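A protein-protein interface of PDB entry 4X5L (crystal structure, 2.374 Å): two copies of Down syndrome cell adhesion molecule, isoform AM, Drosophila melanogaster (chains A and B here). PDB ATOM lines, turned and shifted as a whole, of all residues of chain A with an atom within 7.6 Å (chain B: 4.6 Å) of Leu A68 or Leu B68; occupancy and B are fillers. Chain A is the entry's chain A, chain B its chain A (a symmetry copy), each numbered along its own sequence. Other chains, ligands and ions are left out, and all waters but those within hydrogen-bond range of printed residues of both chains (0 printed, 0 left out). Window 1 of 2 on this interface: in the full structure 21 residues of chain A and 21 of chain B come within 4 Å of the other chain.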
ATOM      1  N   ALA A  26     -26.359  -9.362  17.262  1.00  0.00           N
ATOM      2  CA  ALA A  26     -25.982  -8.523  16.129  1.00  0.00           C
ATOM      3  C   ALA A  26     -24.555  -8.034  16.314  1.00  0.00           C
ATOM      4  O   ALA A  26     -24.112  -7.799  17.438  1.00  0.00           O
ATOM      5  CB  ALA A  26     -26.932  -7.350  15.983  1.00  0.00           C
ATOM      6  N   SER A  27     -23.842  -7.880  15.205  1.00  0.00           N
ATOM      7  CA  SER A  27     -22.443  -7.480  15.252  1.00  0.00           C
ATOM      8  C   SER A  27     -22.059  -6.658  14.027  1.00  0.00           C
ATOM      9  O   SER A  27     -22.376  -7.024  12.894  1.00  0.00           O
ATOM     10  CB  SER A  27     -21.546  -8.712  15.361  1.00  0.00           C
ATOM     11  OG  SER A  27     -20.176  -8.351  15.381  1.00  0.00           O
ATOM     12  N   ALA A  28     -21.376  -5.543  14.270  1.00  0.00           N
ATOM     13  CA  ALA A  28     -20.904  -4.668  13.206  1.00  0.00           C
ATOM     14  C   ALA A  28     -19.458  -4.268  13.469  1.00  0.00           C
ATOM     15  O   ALA A  28     -19.038  -4.155  14.621  1.00  0.00           O
ATOM     16  CB  ALA A  28     -21.787  -3.441  13.096  1.00  0.00           C
ATOM     17  N   ASN A  29     -18.707  -4.052  12.393  1.00  0.00           N
ATOM     18  CA  ASN A  29     -17.278  -3.776  12.488  1.00  0.00           C
ATOM     19  C   ASN A  29     -16.881  -2.493  11.768  1.00  0.00           C
ATOM     20  O   ASN A  29     -16.976  -2.406  10.544  1.00  0.00           O
ATOM     21  CB  ASN A  29     -16.484  -4.949  11.919  1.00  0.00           C
ATOM     22  CG  ASN A  29     -14.990  -4.747  12.031  1.00  0.00           C
ATOM     23  OD1 ASN A  29     -14.501  -4.151  12.992  1.00  0.00           O
ATOM     24  ND2 ASN A  29     -14.252  -5.237  11.043  1.00  0.00           N
ATOM     25  N   CYS A  30     -16.433  -1.503  12.535  1.00  0.00           N
ATOM     26  CA  CYS A  30     -15.942  -0.250  11.975  1.00  0.00           C
ATOM     27  C   CYS A  30     -14.426  -0.302  11.816  1.00  0.00           C
ATOM     28  O   CYS A  30     -13.702  -0.502  12.792  1.00  0.00           O
ATOM     29  CB  CYS A  30     -16.340   0.931  12.862  1.00  0.00           C
ATOM     30  SG  CYS A  30     -15.739   2.531  12.273  1.00  0.00           S
ATOM     31  N   VAL A  31     -13.955  -0.119  10.585  1.00  0.00           N
ATOM     32  CA  VAL A  31     -12.530  -0.201  10.278  1.00  0.00           C
ATOM     33  C   VAL A  31     -12.038   1.109   9.666  1.00  0.00           C
ATOM     34  O   VAL A  31     -12.667   1.653   8.758  1.00  0.00           O
ATOM     35  CB  VAL A  31     -12.230  -1.363   9.311  1.00  0.00           C
ATOM     36  CG1 VAL A  31     -10.728  -1.567   9.167  1.00  0.00           C
ATOM     37  CG2 VAL A  31     -12.891  -2.644   9.804  1.00  0.00           C
ATOM     38  N   ILE A  41     -13.004   6.999  17.792  1.00  0.00           N
ATOM     39  CA  ILE A  41     -14.025   6.181  17.143  1.00  0.00           C
ATOM     40  C   ILE A  41     -15.197   5.954  18.097  1.00  0.00           C
ATOM     41  O   ILE A  41     -15.037   5.353  19.160  1.00  0.00           O
ATOM     42  CB  ILE A  41     -13.450   4.828  16.678  1.00  0.00           C
ATOM     43  CG1 ILE A  41     -12.271   5.059  15.726  1.00  0.00           C
ATOM     44  CG2 ILE A  41     -14.528   3.998  15.989  1.00  0.00           C
ATOM     45  CD1 ILE A  41     -11.517   3.801  15.336  1.00  0.00           C
ATOM     46  N   TRP A  43     -19.625   5.120  18.533  1.00  0.00           N
ATOM     47  CA  TRP A  43     -20.835   4.519  17.975  1.00  0.00           C
ATOM     48  C   TRP A  43     -22.086   5.215  18.499  1.00  0.00           C
ATOM     49  O   TRP A  43     -22.148   5.597  19.668  1.00  0.00           O
ATOM     50  CB  TRP A  43     -20.902   3.029  18.312  1.00  0.00           C
ATOM     51  CG  TRP A  43     -19.936   2.187  17.544  1.00  0.00           C
ATOM     52  CD1 TRP A  43     -18.614   1.996  17.820  1.00  0.00           C
ATOM     53  CD2 TRP A  43     -20.220   1.412  16.374  1.00  0.00           C
ATOM     54  NE1 TRP A  43     -18.055   1.151  16.892  1.00  0.00           N
ATOM     55  CE2 TRP A  43     -19.020   0.779  15.993  1.00  0.00           C
ATOM     56  CE3 TRP A  43     -21.371   1.192  15.610  1.00  0.00           C
ATOM     57  CZ2 TRP A  43     -18.939  -0.058  14.882  1.00  0.00           C
ATOM     58  CZ3 TRP A  43     -21.287   0.361  14.508  1.00  0.00           C
ATOM     59  CH2 TRP A  43     -20.080  -0.253  14.155  1.00  0.00           C
ATOM     60  N   ASN A  52     -20.219   1.535  26.111  1.00  0.00           N
ATOM     61  CA  ASN A  52     -19.886   0.184  26.536  1.00  0.00           C
ATOM     62  C   ASN A  52     -20.464  -0.137  27.909  1.00  0.00           C
ATOM     63  O   ASN A  52     -20.031   0.419  28.918  1.00  0.00           O
ATOM     64  CB  ASN A  52     -18.371  -0.014  26.566  1.00  0.00           C
ATOM     65  CG  ASN A  52     -17.983  -1.438  26.904  1.00  0.00           C
ATOM     66  OD1 ASN A  52     -17.829  -2.278  26.020  1.00  0.00           O
ATOM     67  ND2 ASN A  52     -17.845  -1.720  28.192  1.00  0.00           N
ATOM     68  N   THR A  58     -21.993  -3.639  23.571  1.00  0.00           N
ATOM     69  CA  THR A  58     -20.646  -4.068  23.932  1.00  0.00           C
ATOM     70  C   THR A  58     -19.636  -3.550  22.908  1.00  0.00           C
ATOM     71  O   THR A  58     -19.514  -4.102  21.815  1.00  0.00           O
ATOM     72  CB  THR A  58     -20.548  -5.604  24.017  1.00  0.00           C
ATOM     73  OG1 THR A  58     -21.479  -6.094  24.990  1.00  0.00           O
ATOM     74  CG2 THR A  58     -19.140  -6.044  24.403  1.00  0.00           C
ATOM     75  N   LEU A  59     -18.918  -2.491  23.271  1.00  0.00           N
ATOM     76  CA  LEU A  59     -17.926  -1.885  22.387  1.00  0.00           C
ATOM     77  C   LEU A  59     -16.531  -2.412  22.699  1.00  0.00           C
ATOM     78  O   LEU A  59     -16.167  -2.564  23.862  1.00  0.00           O
ATOM     79  CB  LEU A  59     -17.958  -0.362  22.517  1.00  0.00           C
ATOM     80  CG  LEU A  59     -18.996   0.353  21.649  1.00  0.00           C
ATOM     81  CD1 LEU A  59     -20.379  -0.272  21.792  1.00  0.00           C
ATOM     82  CD2 LEU A  59     -19.041   1.829  22.002  1.00  0.00           C
ATOM     83  N   VAL A  60     -15.749  -2.680  21.656  1.00  0.00           N
ATOM     84  CA  VAL A  60     -14.440  -3.299  21.832  1.00  0.00           C
ATOM     85  C   VAL A  60     -13.419  -2.727  20.851  1.00  0.00           C
ATOM     86  O   VAL A  60     -13.332  -3.154  19.700  1.00  0.00           O
ATOM     87  CB  VAL A  60     -14.535  -4.836  21.670  1.00  0.00           C
ATOM     88  CG1 VAL A  60     -13.154  -5.490  21.722  1.00  0.00           C
ATOM     89  CG2 VAL A  60     -15.439  -5.417  22.758  1.00  0.00           C
ATOM     90  N   ARG A  61     -12.653  -1.749  21.325  1.00  0.00           N
ATOM     91  CA  ARG A  61     -11.540  -1.203  20.561  1.00  0.00           C
ATOM     92  C   ARG A  61     -10.441  -2.257  20.463  1.00  0.00           C
ATOM     93  O   ARG A  61      -9.440  -2.209  21.177  1.00  0.00           O
ATOM     94  CB  ARG A  61     -11.017   0.083  21.210  1.00  0.00           C
ATOM     95  CG  ARG A  61     -11.493   1.361  20.539  1.00  0.00           C
ATOM     96  CD  ARG A  61     -10.587   1.741  19.380  1.00  0.00           C
ATOM     97  NE  ARG A  61     -10.868   3.081  18.877  1.00  0.00           N
ATOM     98  CZ  ARG A  61     -10.424   4.203  19.437  1.00  0.00           C
ATOM     99  NH1 ARG A  61      -9.680   4.158  20.536  1.00  0.00           N
ATOM    100  NH2 ARG A  61     -10.731   5.375  18.902  1.00  0.00           N
ATOM    101  N   LEU A  62     -10.653  -3.225  19.579  1.00  0.00           N
ATOM    102  CA  LEU A  62      -9.710  -4.321  19.386  1.00  0.00           C
ATOM    103  C   LEU A  62      -8.406  -3.822  18.768  1.00  0.00           C
ATOM    104  O   LEU A  62      -7.380  -4.502  18.821  1.00  0.00           O
ATOM    105  CB  LEU A  62     -10.341  -5.397  18.502  1.00  0.00           C
ATOM    106  CG  LEU A  62      -9.637  -6.750  18.412  1.00  0.00           C
ATOM    107  CD1 LEU A  62     -10.681  -7.848  18.468  1.00  0.00           C
ATOM    108  CD2 LEU A  62      -8.815  -6.859  17.136  1.00  0.00           C
ATOM    109  N   ASN A  63      -8.457  -2.627  18.189  1.00  0.00           N
ATOM    110  CA  ASN A  63      -7.301  -2.027  17.540  1.00  0.00           C
ATOM    111  C   ASN A  63      -7.422  -0.508  17.553  1.00  0.00           C
ATOM    112  O   ASN A  63      -8.497   0.030  17.817  1.00  0.00           O
ATOM    113  CB  ASN A  63      -7.174  -2.537  16.103  1.00  0.00           C
ATOM    114  CG  ASN A  63      -5.885  -2.100  15.435  1.00  0.00           C
ATOM    115  OD1 ASN A  63      -5.762  -0.959  14.987  1.00  0.00           O
ATOM    116  ND2 ASN A  63      -4.921  -3.009  15.355  1.00  0.00           N
ATOM    117  N   THR A  66      -9.658  -0.091  14.648  1.00  0.00           N
ATOM    118  CA  THR A  66     -10.849  -0.931  14.612  1.00  0.00           C
ATOM    119  C   THR A  66     -11.710  -0.766  15.857  1.00  0.00           C
ATOM    120  O   THR A  66     -11.202  -0.654  16.971  1.00  0.00           O
ATOM    121  CB  THR A  66     -10.488  -2.421  14.477  1.00  0.00           C
ATOM    122  OG1 THR A  66      -9.617  -2.607  13.355  1.00  0.00           O
ATOM    123  CG2 THR A  66     -11.748  -3.265  14.286  1.00  0.00           C
ATOM    124  N   SER A  67     -13.022  -0.768  15.646  1.00  0.00           N
ATOM    125  CA  SER A  67     -13.986  -0.711  16.735  1.00  0.00           C
ATOM    126  C   SER A  67     -15.189  -1.598  16.442  1.00  0.00           C
ATOM    127  O   SER A  67     -16.064  -1.225  15.661  1.00  0.00           O
ATOM    128  CB  SER A  67     -14.442   0.727  16.965  1.00  0.00           C
ATOM    129  OG  SER A  67     -15.490   0.779  17.914  1.00  0.00           O
ATOM    130  N   LEU A  68     -15.230  -2.770  17.068  1.00  0.00           N
ATOM    131  CA  LEU A  68     -16.352  -3.681  16.896  1.00  0.00           C
ATOM    132  C   LEU A  68     -17.465  -3.351  17.878  1.00  0.00           C
ATOM    133  O   LEU A  68     -17.212  -3.111  19.058  1.00  0.00           O
ATOM    134  CB  LEU A  68     -15.912  -5.137  17.082  1.00  0.00           C
ATOM    135  CG  LEU A  68     -17.031  -6.175  16.953  1.00  0.00           C
ATOM    136  CD1 LEU A  68     -16.506  -7.448  16.311  1.00  0.00           C
ATOM    137  CD2 LEU A  68     -17.656  -6.481  18.310  1.00  0.00           C
ATOM    138  N   LEU A  69     -18.696  -3.354  17.379  1.00  0.00           N
ATOM    139  CA  LEU A  69     -19.872  -3.235  18.226  1.00  0.00           C
ATOM    140  C   LEU A  69     -20.599  -4.560  18.221  1.00  0.00           C
ATOM    141  O   LEU A  69     -20.739  -5.196  17.176  1.00  0.00           O
ATOM    142  CB  LEU A  69     -20.798  -2.114  17.744  1.00  0.00           C
ATOM    143  CG  LEU A  69     -22.139  -1.984  18.476  1.00  0.00           C
ATOM    144  CD1 LEU A  69     -22.500  -0.522  18.654  1.00  0.00           C
ATOM    145  CD2 LEU A  69     -23.247  -2.707  17.720  1.00  0.00           C
ATOM    146  N   ASN A  70     -21.052  -4.976  19.397  1.00  0.00           N
ATOM    147  CA  ASN A  70     -21.772  -6.228  19.531  1.00  0.00           C
ATOM    148  C   ASN A  70     -23.041  -6.084  20.363  1.00  0.00           C
ATOM    149  O   ASN A  70     -23.110  -5.260  21.272  1.00  0.00           O
ATOM    150  CB  ASN A  70     -20.872  -7.285  20.162  1.00  0.00           C
ATOM    151  CG  ASN A  70     -21.559  -8.627  20.282  1.00  0.00           C
ATOM    152  OD1 ASN A  70     -22.375  -8.842  21.175  1.00  0.00           O
ATOM    153  ND2 ASN A  70     -21.242  -9.536  19.373  1.00  0.00           N
ATOM    154  N   ILE A  71     -24.039  -6.903  20.036  1.00  0.00           N
ATOM    155  CA  ILE A  71     -25.272  -6.986  20.812  1.00  0.00           C
ATOM    156  C   ILE A  71     -25.578  -8.461  21.054  1.00  0.00           C
ATOM    157  O   ILE A  71     -25.658  -9.243  20.108  1.00  0.00           O
ATOM    158  CB  ILE A  71     -26.463  -6.304  20.097  1.00  0.00           C
ATOM    159  CG1 ILE A  71     -26.082  -4.884  19.661  1.00  0.00           C
ATOM    160  CG2 ILE A  71     -27.690  -6.279  21.010  1.00  0.00           C
ATOM    161  CD1 ILE A  71     -27.112  -4.206  18.781  1.00  0.00           C
ATOM    162  N   CYS A  84     -20.820   4.954  12.762  1.00  0.00           N
ATOM    163  CA  CYS A  84     -19.476   4.887  13.327  1.00  0.00           C
ATOM    164  C   CYS A  84     -18.633   6.047  12.805  1.00  0.00           C
ATOM    165  O   CYS A  84     -18.298   6.088  11.623  1.00  0.00           O
ATOM    166  CB  CYS A  84     -18.811   3.555  12.983  1.00  0.00           C
ATOM    167  SG  CYS A  84     -17.084   3.439  13.493  1.00  0.00           S
ATOM    168  N   SER B  27      -9.724  -6.030   8.437  1.00  0.00           N
ATOM    169  CA  SER B  27     -10.587  -6.601   9.461  1.00  0.00           C
ATOM    170  C   SER B  27     -11.885  -7.132   8.861  1.00  0.00           C
ATOM    171  O   SER B  27     -12.535  -6.457   8.060  1.00  0.00           O
ATOM    172  CB  SER B  27     -10.892  -5.557  10.534  1.00  0.00           C
ATOM    173  OG  SER B  27     -11.754  -6.080  11.529  1.00  0.00           O
ATOM    174  N   ALA B  28     -12.248  -8.348   9.256  1.00  0.00           N
ATOM    175  CA  ALA B  28     -13.479  -8.982   8.803  1.00  0.00           C
ATOM    176  C   ALA B  28     -14.201  -9.612   9.987  1.00  0.00           C
ATOM    177  O   ALA B  28     -13.567 -10.061  10.942  1.00  0.00           O
ATOM    178  CB  ALA B  28     -13.182 -10.022   7.742  1.00  0.00           C
ATOM    179  N   ASN B  29     -15.528  -9.645   9.911  1.00  0.00           N
ATOM    180  CA  ASN B  29     -16.356 -10.112  11.017  1.00  0.00           C
ATOM    181  C   ASN B  29     -17.323 -11.214  10.599  1.00  0.00           C
ATOM    182  O   ASN B  29     -18.236 -10.980   9.808  1.00  0.00           O
ATOM    183  CB  ASN B  29     -17.139  -8.943  11.610  1.00  0.00           C
ATOM    184  CG  ASN B  29     -17.984  -9.352  12.795  1.00  0.00           C
ATOM    185  OD1 ASN B  29     -17.601 -10.225  13.575  1.00  0.00           O
ATOM    186  ND2 ASN B  29     -19.146  -8.726  12.935  1.00  0.00           N
ATOM    187  N   THR B  58      -4.816 -12.424  13.576  1.00  0.00           N
ATOM    188  CA  THR B  58      -5.297 -12.271  14.945  1.00  0.00           C
ATOM    189  C   THR B  58      -6.778 -12.638  15.027  1.00  0.00           C
ATOM    190  O   THR B  58      -7.642 -11.850  14.640  1.00  0.00           O
ATOM    191  CB  THR B  58      -5.098 -10.829  15.454  1.00  0.00           C
ATOM    192  OG1 THR B  58      -3.708 -10.485  15.399  1.00  0.00           O
ATOM    193  CG2 THR B  58      -5.596 -10.679  16.888  1.00  0.00           C
ATOM    194  N   LEU B  59      -7.062 -13.835  15.531  1.00  0.00           N
ATOM    195  CA  LEU B  59      -8.435 -14.320  15.656  1.00  0.00           C
ATOM    196  C   LEU B  59      -8.972 -14.067  17.058  1.00  0.00           C
ATOM    197  O   LEU B  59      -8.261 -14.257  18.043  1.00  0.00           O
ATOM    198  CB  LEU B  59      -8.504 -15.811  15.324  1.00  0.00           C
ATOM    199  CG  LEU B  59      -8.643 -16.151  13.839  1.00  0.00           C
ATOM    200  CD1 LEU B  59      -7.613 -15.414  12.991  1.00  0.00           C
ATOM    201  CD2 LEU B  59      -8.524 -17.651  13.635  1.00  0.00           C
ATOM    202  N   VAL B  60     -10.231 -13.647  17.147  1.00  0.00           N
ATOM    203  CA  VAL B  60     -10.811 -13.260  18.428  1.00  0.00           C
ATOM    204  C   VAL B  60     -12.273 -13.691  18.529  1.00  0.00           C
ATOM    205  O   VAL B  60     -13.175 -13.005  18.051  1.00  0.00           O
ATOM    206  CB  VAL B  60     -10.688 -11.732  18.646  1.00  0.00           C
ATOM    207  CG1 VAL B  60     -11.405 -11.290  19.923  1.00  0.00           C
ATOM    208  CG2 VAL B  60      -9.213 -11.333  18.701  1.00  0.00           C
ATOM    209  N   LEU B  62     -14.889 -13.242  20.102  1.00  0.00           N
ATOM    210  CA  LEU B  62     -15.476 -12.259  21.005  1.00  0.00           C
ATOM    211  C   LEU B  62     -16.815 -12.746  21.552  1.00  0.00           C
ATOM    212  O   LEU B  62     -17.312 -12.235  22.558  1.00  0.00           O
ATOM    213  CB  LEU B  62     -15.651 -10.926  20.277  1.00  0.00           C
ATOM    214  CG  LEU B  62     -15.981  -9.692  21.117  1.00  0.00           C
ATOM    215  CD1 LEU B  62     -15.165  -8.521  20.604  1.00  0.00           C
ATOM    216  CD2 LEU B  62     -17.467  -9.372  21.064  1.00  0.00           C
ATOM    217  N   THR B  66     -19.752 -15.143  17.299  1.00  0.00           N
ATOM    218  CA  THR B  66     -18.952 -14.178  16.554  1.00  0.00           C
ATOM    219  C   THR B  66     -17.473 -14.541  16.544  1.00  0.00           C
ATOM    220  O   THR B  66     -16.922 -14.989  17.548  1.00  0.00           O
ATOM    221  CB  THR B  66     -19.091 -12.759  17.133  1.00  0.00           C
ATOM    222  OG1 THR B  66     -20.477 -12.409  17.226  1.00  0.00           O
ATOM    223  CG2 THR B  66     -18.370 -11.744  16.248  1.00  0.00           C
ATOM    224  N   SER B  67     -16.841 -14.321  15.396  1.00  0.00           N
ATOM    225  CA  SER B  67     -15.408 -14.528  15.245  1.00  0.00           C
ATOM    226  C   SER B  67     -14.797 -13.453  14.356  1.00  0.00           C
ATOM    227  O   SER B  67     -14.924 -13.506  13.133  1.00  0.00           O
ATOM    228  CB  SER B  67     -15.131 -15.909  14.657  1.00  0.00           C
ATOM    229  OG  SER B  67     -13.756 -16.065  14.361  1.00  0.00           O
ATOM    230  N   LEU B  68     -14.134 -12.479  14.972  1.00  0.00           N
ATOM    231  CA  LEU B  68     -13.473 -11.421  14.222  1.00  0.00           C
ATOM    232  C   LEU B  68     -12.068 -11.843  13.824  1.00  0.00           C
ATOM    233  O   LEU B  68     -11.326 -12.401  14.633  1.00  0.00           O
ATOM    234  CB  LEU B  68     -13.413 -10.125  15.036  1.00  0.00           C
ATOM    235  CG  LEU B  68     -12.704  -8.955  14.345  1.00  0.00           C
ATOM    236  CD1 LEU B  68     -13.368  -7.638  14.711  1.00  0.00           C
ATOM    237  CD2 LEU B  68     -11.222  -8.922  14.702  1.00  0.00           C
ATOM    238  N   LEU B  69     -11.711 -11.562  12.576  1.00  0.00           N
ATOM    239  CA  LEU B  69     -10.347 -11.741  12.104  1.00  0.00           C
ATOM    240  C   LEU B  69      -9.744 -10.376  11.863  1.00  0.00           C
ATOM    241  O   LEU B  69     -10.398  -9.488  11.319  1.00  0.00           O
ATOM    242  CB  LEU B  69     -10.303 -12.581  10.825  1.00  0.00           C
ATOM    243  CG  LEU B  69      -8.930 -12.721  10.156  1.00  0.00           C
ATOM    244  CD1 LEU B  69      -8.754 -14.124   9.608  1.00  0.00           C
ATOM    245  CD2 LEU B  69      -8.760 -11.700   9.038  1.00  0.00           C
ATOM    246  N   ASN B  70      -8.495 -10.215  12.279  1.00  0.00           N
ATOM    247  CA  ASN B  70      -7.795  -8.956  12.104  1.00  0.00           C
ATOM    248  C   ASN B  70      -6.390  -9.143  11.545  1.00  0.00           C
ATOM    249  O   ASN B  70      -5.737 -10.154  11.800  1.00  0.00           O
ATOM    250  CB  ASN B  70      -7.715  -8.212  13.431  1.00  0.00           C
ATOM    251  CG  ASN B  70      -7.036  -6.867  13.297  1.00  0.00           C
ATOM    252  OD1 ASN B  70      -5.812  -6.782  13.217  1.00  0.00           O
ATOM    253  ND2 ASN B  70      -7.827  -5.806  13.257  1.00  0.00           N
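Of the printed residues of chain B, Ser A27 touches Asn B29 (2.7 Å) and Thr B66 (3.9 Å). Printed residues of chain B within 4 Å of Val A60: Leu B62. Of the printed residues of chain B, Thr A66 touches Ser B27 and Asn B70. Printed residues of chain B within 4 Å of Leu A68: Leu B62 and Leu B68. Printed residues of chain A within 4 Å of Val B60: Leu A62 (3.8 Å). Printed residues of chain A within 4 Å of Leu B62: Val A60 (3.8 Å) and Leu A68 (3.95 Å). Of chain A, only Leu A62 (3.95 Å) and Leu A68 (3.5 Å) come within 4 Å of Leu B68. The nearest residue of chain B that does not touch Leu A68 is Asn B29 (4.05 Å). The nearest residue of chain A that does not touch Leu B68 is Asn A29 (4.05 Å).
Among the printed residues, pairs that only touch across the chains: Leu A68 with Leu B68 (3.5 Å), Val A31 with Ser B27 (3.6 Å), Thr A66 with Asn B70 (3.7 Å), Asn A70 with Thr B66 (3.7 Å), Val A60 with Leu B62 (3.8 Å), Leu A62 with Val B60 (3.8 Å), Thr A66 with Ser B27 (3.9 Å), Ser A27 with Thr B66 (3.9 Å), Leu A62 with Leu B68 (3.95 Å) and Leu A68 with Leu B62 (3.95 Å).
The backbone carbonyl oxygen (O) of Thr A58 lies within hydrogen-bond range of the backbone NH (N) of Asn A70 (3.0 Å). The backbone NH (N) of Val A60 lies within hydrogen-bond range of the backbone carbonyl oxygen (O) of Leu A68 (3.0 Å). The backbone NH (N) of Asn B70 sits at hydrogen-bond distance from the backbone carbonyl oxygen (O) of Thr B58. The backbone NH (N) of Val B60 sits at hydrogen-bond distance from the backbone carbonyl oxygen (O) of Leu B68, at 3.0 Å. The side-chain sulfur (SG) of Cys A30 forms a disulfide with the side-chain sulfur (SG) of Cys A84.
Ser A27 touches Asn B29, and with the chains exchanged Asn A29 touches Ser B27. Ser A27 touches Thr B66, and with the chains exchanged Thr A66 touches Ser B27. Val A60 touches Leu B62, and with the chains exchanged Leu A62 touches Val B60. Leu A62 touches Leu B68, and with the chains exchanged Leu A68 touches Leu B62. Of the 12 pairs that touch across the chains among the printed residues, 11 have their exchanged pair printed and touching as well.
Of the 22 printed residues of chain A, 8 touch a printed residue of chain B. Hydrophobic or aromatic side chains of chain A within 4 Å of the printed part of chain B: Val A31, Val A60, Leu A62 and Leu A68. Of the 12 printed residues of chain B, 7 touch a printed residue of chain A. Printed residues of chain B that touch a printed residue of chain A: Ser B27, Asn B29, Val B60, Leu B62, Thr B66, Leu B68 and Asn B70. Among the printed residues, no Asp or Glu carboxylate lies within 4 Å of a Lys or Arg side-chain nitrogen of the other chain.
ND2 of Asn B29 sits at hydrogen-bond distance from OG of Ser A27 (2.7 Å). The side-chain amide nitrogen (ND2) of Asn A29 sits at hydrogen-bond distance from the side-chain hydroxyl (OG) of Ser B27 (2.7 Å).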
